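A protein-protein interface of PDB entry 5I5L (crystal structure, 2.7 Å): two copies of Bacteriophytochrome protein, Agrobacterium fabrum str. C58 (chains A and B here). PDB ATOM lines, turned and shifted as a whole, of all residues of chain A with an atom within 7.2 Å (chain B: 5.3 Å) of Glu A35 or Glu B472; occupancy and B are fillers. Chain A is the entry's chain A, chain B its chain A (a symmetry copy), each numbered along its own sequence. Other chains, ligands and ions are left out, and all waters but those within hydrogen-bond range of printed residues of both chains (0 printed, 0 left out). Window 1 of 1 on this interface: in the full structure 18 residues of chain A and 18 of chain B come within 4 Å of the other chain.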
ATOM      1  N   LEU A  31      -7.541  -5.134  24.737  1.00  0.00           N
ATOM      2  CA  LEU A  31      -7.809  -6.518  24.332  1.00  0.00           C
ATOM      3  C   LEU A  31      -9.294  -6.935  24.336  1.00  0.00           C
ATOM      4  O   LEU A  31     -10.133  -6.322  24.997  1.00  0.00           O
ATOM      5  CB  LEU A  31      -6.906  -7.509  25.082  1.00  0.00           C
ATOM      6  CG  LEU A  31      -6.477  -7.254  26.519  1.00  0.00           C
ATOM      7  CD1 LEU A  31      -7.541  -7.765  27.457  1.00  0.00           C
ATOM      8  CD2 LEU A  31      -5.166  -7.963  26.811  1.00  0.00           C
ATOM      9  N   SER A  32      -9.574  -7.979  23.546  1.00  0.00           N
ATOM     10  CA  SER A  32     -10.923  -8.513  23.323  1.00  0.00           C
ATOM     11  C   SER A  32     -11.322  -9.475  24.433  1.00  0.00           C
ATOM     12  O   SER A  32     -10.696 -10.513  24.600  1.00  0.00           O
ATOM     13  CB  SER A  32     -10.998  -9.253  21.984  1.00  0.00           C
ATOM     14  OG  SER A  32     -12.049 -10.208  21.987  1.00  0.00           O
ATOM     15  N   ALA A  33     -12.396  -9.132  25.141  1.00  0.00           N
ATOM     16  CA  ALA A  33     -12.910  -9.884  26.295  1.00  0.00           C
ATOM     17  C   ALA A  33     -13.104 -11.381  26.082  1.00  0.00           C
ATOM     18  O   ALA A  33     -12.845 -12.188  26.985  1.00  0.00           O
ATOM     19  CB  ALA A  33     -14.234  -9.288  26.728  1.00  0.00           C
ATOM     20  N   ARG A  34     -13.590 -11.740  24.900  1.00  0.00           N
ATOM     21  CA  ARG A  34     -13.872 -13.131  24.582  1.00  0.00           C
ATOM     22  C   ARG A  34     -12.626 -13.978  24.840  1.00  0.00           C
ATOM     23  O   ARG A  34     -12.675 -14.931  25.626  1.00  0.00           O
ATOM     24  CB  ARG A  34     -14.373 -13.246  23.126  1.00  0.00           C
ATOM     25  CG  ARG A  34     -15.040 -14.555  22.680  1.00  0.00           C
ATOM     26  CD  ARG A  34     -15.578 -15.477  23.782  1.00  0.00           C
ATOM     27  NE  ARG A  34     -16.606 -14.869  24.637  1.00  0.00           N
ATOM     28  CZ  ARG A  34     -17.889 -14.684  24.306  1.00  0.00           C
ATOM     29  NH1 ARG A  34     -18.716 -14.116  25.185  1.00  0.00           N
ATOM     30  NH2 ARG A  34     -18.365 -15.053  23.116  1.00  0.00           N
ATOM     31  N   GLU A  35     -11.506 -13.565  24.249  1.00  0.00           N
ATOM     32  CA  GLU A  35     -10.279 -14.369  24.230  1.00  0.00           C
ATOM     33  C   GLU A  35      -9.029 -13.713  24.822  1.00  0.00           C
ATOM     34  O   GLU A  35      -7.980 -14.354  24.890  1.00  0.00           O
ATOM     35  CB  GLU A  35      -9.997 -14.747  22.779  1.00  0.00           C
ATOM     36  CG  GLU A  35     -11.186 -15.392  22.073  1.00  0.00           C
ATOM     37  CD  GLU A  35     -11.646 -16.694  22.731  1.00  0.00           C
ATOM     38  OE1 GLU A  35     -10.787 -17.523  23.104  1.00  0.00           O
ATOM     39  OE2 GLU A  35     -12.869 -16.911  22.849  1.00  0.00           O
ATOM     40  N   PHE A  36      -9.143 -12.461  25.267  1.00  0.00           N
ATOM     41  CA  PHE A  36      -7.986 -11.618  25.611  1.00  0.00           C
ATOM     42  C   PHE A  36      -6.908 -11.627  24.527  1.00  0.00           C
ATOM     43  O   PHE A  36      -5.744 -11.931  24.788  1.00  0.00           O
ATOM     44  CB  PHE A  36      -7.402 -11.985  26.983  1.00  0.00           C
ATOM     45  CG  PHE A  36      -8.402 -11.925  28.103  1.00  0.00           C
ATOM     46  CD1 PHE A  36      -9.221 -10.812  28.272  1.00  0.00           C
ATOM     47  CD2 PHE A  36      -8.524 -12.982  28.998  1.00  0.00           C
ATOM     48  CE1 PHE A  36     -10.148 -10.758  29.296  1.00  0.00           C
ATOM     49  CE2 PHE A  36      -9.451 -12.934  30.031  1.00  0.00           C
ATOM     50  CZ  PHE A  36     -10.264 -11.817  30.181  1.00  0.00           C
ATOM     51  N   SER A  37      -7.333 -11.300  23.309  1.00  0.00           N
ATOM     52  CA  SER A  37      -6.429 -11.107  22.184  1.00  0.00           C
ATOM     53  C   SER A  37      -6.194  -9.618  22.005  1.00  0.00           C
ATOM     54  O   SER A  37      -7.095  -8.824  22.236  1.00  0.00           O
ATOM     55  CB  SER A  37      -7.010 -11.713  20.907  1.00  0.00           C
ATOM     56  OG  SER A  37      -8.122 -10.973  20.454  1.00  0.00           O
ATOM     57  N   VAL A  38      -4.991  -9.245  21.583  1.00  0.00           N
ATOM     58  CA  VAL A  38      -4.621  -7.841  21.456  1.00  0.00           C
ATOM     59  C   VAL A  38      -5.292  -7.243  20.235  1.00  0.00           C
ATOM     60  O   VAL A  38      -5.216  -7.800  19.140  1.00  0.00           O
ATOM     61  CB  VAL A  38      -3.097  -7.645  21.350  1.00  0.00           C
ATOM     62  CG1 VAL A  38      -2.749  -6.173  21.113  1.00  0.00           C
ATOM     63  CG2 VAL A  38      -2.417  -8.181  22.605  1.00  0.00           C
ATOM     64  N   ALA A  57      -2.418 -11.264  18.809  1.00  0.00           N
ATOM     65  CA  ALA A  57      -1.746 -12.060  19.836  1.00  0.00           C
ATOM     66  C   ALA A  57      -2.633 -12.250  21.052  1.00  0.00           C
ATOM     67  O   ALA A  57      -3.178 -11.287  21.563  1.00  0.00           O
ATOM     68  CB  ALA A  57      -0.445 -11.397  20.257  1.00  0.00           C
ATOM     69  N   VAL A  58      -2.772 -13.497  21.496  1.00  0.00           N
ATOM     70  CA  VAL A  58      -3.483 -13.829  22.730  1.00  0.00           C
ATOM     71  C   VAL A  58      -2.548 -13.585  23.904  1.00  0.00           C
ATOM     72  O   VAL A  58      -1.365 -13.901  23.830  1.00  0.00           O
ATOM     73  CB  VAL A  58      -4.014 -15.291  22.706  1.00  0.00           C
ATOM     74  CG1 VAL A  58      -4.170 -15.890  24.105  1.00  0.00           C
ATOM     75  CG2 VAL A  58      -5.340 -15.348  21.950  1.00  0.00           C
ATOM     76  N   ALA A  59      -3.095 -13.023  24.979  1.00  0.00           N
ATOM     77  CA  ALA A  59      -2.350 -12.811  26.213  1.00  0.00           C
ATOM     78  C   ALA A  59      -2.198 -14.129  26.976  1.00  0.00           C
ATOM     79  O   ALA A  59      -3.167 -14.886  27.103  1.00  0.00           O
ATOM     80  CB  ALA A  59      -3.062 -11.792  27.074  1.00  0.00           C
ATOM     81  N   ILE A  67      -2.659 -12.129  34.068  1.00  0.00           N
ATOM     82  CA  ILE A  67      -3.743 -12.605  33.195  1.00  0.00           C
ATOM     83  C   ILE A  67      -4.772 -13.473  33.924  1.00  0.00           C
ATOM     84  O   ILE A  67      -5.972 -13.369  33.652  1.00  0.00           O
ATOM     85  CB  ILE A  67      -3.198 -13.345  31.948  1.00  0.00           C
ATOM     86  CG1 ILE A  67      -4.306 -13.627  30.923  1.00  0.00           C
ATOM     87  CG2 ILE A  67      -2.524 -14.656  32.329  1.00  0.00           C
ATOM     88  CD1 ILE A  67      -5.054 -12.403  30.443  1.00  0.00           C
ATOM     89  N   ARG B 309     -15.632 -27.429  22.252  1.00  0.00           N
ATOM     90  CA  ARG B 309     -14.400 -27.355  23.071  1.00  0.00           C
ATOM     91  C   ARG B 309     -14.039 -28.689  23.732  1.00  0.00           C
ATOM     92  O   ARG B 309     -12.861 -29.080  23.767  1.00  0.00           O
ATOM     93  CB  ARG B 309     -14.485 -26.241  24.138  1.00  0.00           C
ATOM     94  CG  ARG B 309     -14.269 -24.854  23.551  1.00  0.00           C
ATOM     95  CD  ARG B 309     -13.996 -23.758  24.565  1.00  0.00           C
ATOM     96  NE  ARG B 309     -14.086 -22.449  23.898  1.00  0.00           N
ATOM     97  CZ  ARG B 309     -13.063 -21.702  23.466  1.00  0.00           C
ATOM     98  NH1 ARG B 309     -11.797 -22.065  23.655  1.00  0.00           N
ATOM     99  NH2 ARG B 309     -13.311 -20.543  22.861  1.00  0.00           N
ATOM    100  N   TRP B 470     -12.007 -20.309  10.726  1.00  0.00           N
ATOM    101  CA  TRP B 470     -11.563 -21.068  11.874  1.00  0.00           C
ATOM    102  C   TRP B 470     -12.368 -20.587  13.065  1.00  0.00           C
ATOM    103  O   TRP B 470     -12.437 -19.388  13.318  1.00  0.00           O
ATOM    104  CB  TRP B 470     -10.065 -20.881  12.116  1.00  0.00           C
ATOM    105  CG  TRP B 470      -9.214 -21.230  10.919  1.00  0.00           C
ATOM    106  CD1 TRP B 470      -8.758 -20.364   9.957  1.00  0.00           C
ATOM    107  CD2 TRP B 470      -8.728 -22.525  10.549  1.00  0.00           C
ATOM    108  NE1 TRP B 470      -8.019 -21.037   9.024  1.00  0.00           N
ATOM    109  CE2 TRP B 470      -7.984 -22.367   9.358  1.00  0.00           C
ATOM    110  CE3 TRP B 470      -8.844 -23.802  11.105  1.00  0.00           C
ATOM    111  CZ2 TRP B 470      -7.353 -23.445   8.714  1.00  0.00           C
ATOM    112  CZ3 TRP B 470      -8.210 -24.867  10.466  1.00  0.00           C
ATOM    113  CH2 TRP B 470      -7.475 -24.678   9.280  1.00  0.00           C
ATOM    114  N   SER B 471     -12.999 -21.527  13.768  1.00  0.00           N
ATOM    115  CA  SER B 471     -13.726 -21.220  14.985  1.00  0.00           C
ATOM    116  C   SER B 471     -12.738 -20.978  16.110  1.00  0.00           C
ATOM    117  O   SER B 471     -11.614 -21.460  16.084  1.00  0.00           O
ATOM    118  CB  SER B 471     -14.712 -22.347  15.335  1.00  0.00           C
ATOM    119  OG  SER B 471     -14.091 -23.492  15.908  1.00  0.00           O
ATOM    120  N   GLU B 472     -13.164 -20.224  17.109  1.00  0.00           N
ATOM    121  CA  GLU B 472     -12.304 -19.908  18.258  1.00  0.00           C
ATOM    122  C   GLU B 472     -11.901 -21.106  19.143  1.00  0.00           C
ATOM    123  O   GLU B 472     -10.843 -21.056  19.771  1.00  0.00           O
ATOM    124  CB  GLU B 472     -12.930 -18.788  19.107  1.00  0.00           C
ATOM    125  CG  GLU B 472     -11.946 -18.069  20.024  1.00  0.00           C
ATOM    126  CD  GLU B 472     -10.729 -17.477  19.305  1.00  0.00           C
ATOM    127  OE1 GLU B 472      -9.595 -17.907  19.623  1.00  0.00           O
ATOM    128  OE2 GLU B 472     -10.907 -16.589  18.430  1.00  0.00           O
ATOM    129  N   PRO B 473     -12.747 -22.159  19.214  1.00  0.00           N
ATOM    130  CA  PRO B 473     -12.303 -23.422  19.811  1.00  0.00           C
ATOM    131  C   PRO B 473     -11.171 -24.087  19.043  1.00  0.00           C
ATOM    132  O   PRO B 473     -10.270 -24.667  19.652  1.00  0.00           O
ATOM    133  CB  PRO B 473     -13.555 -24.304  19.748  1.00  0.00           C
ATOM    134  CG  PRO B 473     -14.687 -23.346  19.789  1.00  0.00           C
ATOM    135  CD  PRO B 473     -14.211 -22.138  19.033  1.00  0.00           C
ATOM    136  N   GLU B 474     -11.230 -23.999  17.714  1.00  0.00           N
ATOM    137  CA  GLU B 474     -10.202 -24.566  16.849  1.00  0.00           C
ATOM    138  C   GLU B 474      -8.867 -23.856  17.018  1.00  0.00           C
ATOM    139  O   GLU B 474      -7.846 -24.520  17.140  1.00  0.00           O
ATOM    140  CB  GLU B 474     -10.667 -24.571  15.391  1.00  0.00           C
ATOM    141  CG  GLU B 474     -11.773 -25.587  15.154  1.00  0.00           C
ATOM    142  CD  GLU B 474     -12.519 -25.427  13.835  1.00  0.00           C
ATOM    143  OE1 GLU B 474     -12.464 -24.345  13.188  1.00  0.00           O
ATOM    144  OE2 GLU B 474     -13.185 -26.419  13.446  1.00  0.00           O
ATOM    145  N   LEU B 475      -8.865 -22.525  17.062  1.00  0.00           N
ATOM    146  CA  LEU B 475      -7.618 -21.779  17.287  1.00  0.00           C
ATOM    147  C   LEU B 475      -7.087 -22.007  18.703  1.00  0.00           C
ATOM    148  O   LEU B 475      -5.876 -22.010  18.938  1.00  0.00           O
ATOM    149  CB  LEU B 475      -7.812 -20.274  17.064  1.00  0.00           C
ATOM    150  CG  LEU B 475      -8.299 -19.738  15.709  1.00  0.00           C
ATOM    151  CD1 LEU B 475      -8.271 -18.217  15.689  1.00  0.00           C
ATOM    152  CD2 LEU B 475      -7.474 -20.273  14.560  1.00  0.00           C
ATOM    153  N   ALA B 476      -8.002 -22.179  19.650  1.00  0.00           N
ATOM    154  CA  ALA B 476      -7.633 -22.453  21.019  1.00  0.00           C
ATOM    155  C   ALA B 476      -6.914 -23.794  21.102  1.00  0.00           C
ATOM    156  O   ALA B 476      -5.875 -23.897  21.752  1.00  0.00           O
ATOM    157  CB  ALA B 476      -8.859 -22.442  21.904  1.00  0.00           C
ATOM    158  N   ALA B 477      -7.450 -24.809  20.426  1.00  0.00           N
ATOM    159  CA  ALA B 477      -6.795 -26.134  20.360  1.00  0.00           C
ATOM    160  C   ALA B 477      -5.440 -26.072  19.686  1.00  0.00           C
ATOM    161  O   ALA B 477      -4.517 -26.778  20.097  1.00  0.00           O
ATOM    162  CB  ALA B 477      -7.672 -27.135  19.632  1.00  0.00           C
ATOM    163  N   ARG B 479      -3.317 -23.387  19.583  1.00  0.00           N
ATOM    164  CA  ARG B 479      -2.414 -22.806  20.586  1.00  0.00           C
ATOM    165  C   ARG B 479      -2.092 -23.809  21.697  1.00  0.00           C
ATOM    166  O   ARG B 479      -0.931 -23.943  22.085  1.00  0.00           O
ATOM    167  CB  ARG B 479      -2.997 -21.511  21.178  1.00  0.00           C
ATOM    168  CG  ARG B 479      -2.901 -20.322  20.232  1.00  0.00           C
ATOM    169  CD  ARG B 479      -3.328 -19.008  20.869  1.00  0.00           C
ATOM    170  NE  ARG B 479      -4.784 -18.904  20.967  1.00  0.00           N
ATOM    171  CZ  ARG B 479      -5.602 -18.386  20.043  1.00  0.00           C
ATOM    172  NH1 ARG B 479      -5.148 -17.881  18.887  1.00  0.00           N
ATOM    173  NH2 ARG B 479      -6.910 -18.370  20.283  1.00  0.00           N
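Glu B472 touches just one residue of chain A: Glu A35. Of the printed residues of chain A, Arg B309 touches Glu A35 (3.7 Å). Printed residues of chain B within 4 Å of Val A58: Arg B479 (3.6 Å). Of the printed residues of chain A, Arg B479 touches Val A58 (3.6 Å). Ser B471 touches none of the printed residues of chain A. Ser A32 touches none of the printed residues of chain B. The nearest residue of chain A that does not touch Glu B472 is Arg A34 (5.4 Å). The nearest printed residue of chain B that does not touch Val A58 is Glu B472 (5.5 Å).
No position is printed for both chains. Of the 3 pairs that touch across the chains among the printed residues, none has its exchanged pair printed and touching as well.
NH2 of Arg B479 lies within salt-bridge range of OE1 of Glu B472 (2.8 Å).
CG of Glu B472 touches CD of Glu A35 (3.1 Å). CG2 of Val A58 touches CZ of Arg B479, 3.6 Å away.
Of the 12 printed residues of chain A, 2 touch a printed residue of chain B. Hydrophobic or aromatic side chains of chain A that line the printed part of chain B: Val A58. Printed residues of chain B that touch a printed residue of chain A: Arg B309, Glu B472 and Arg B479. Along chain B the printed residues that touch a printed residue of chain A span positions 309 to 479.
The guanidinium group (NH2) of Arg B309 lies within salt-bridge range of the side-chain carboxylate (OE2) of Glu A35, 3.7 Å away.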
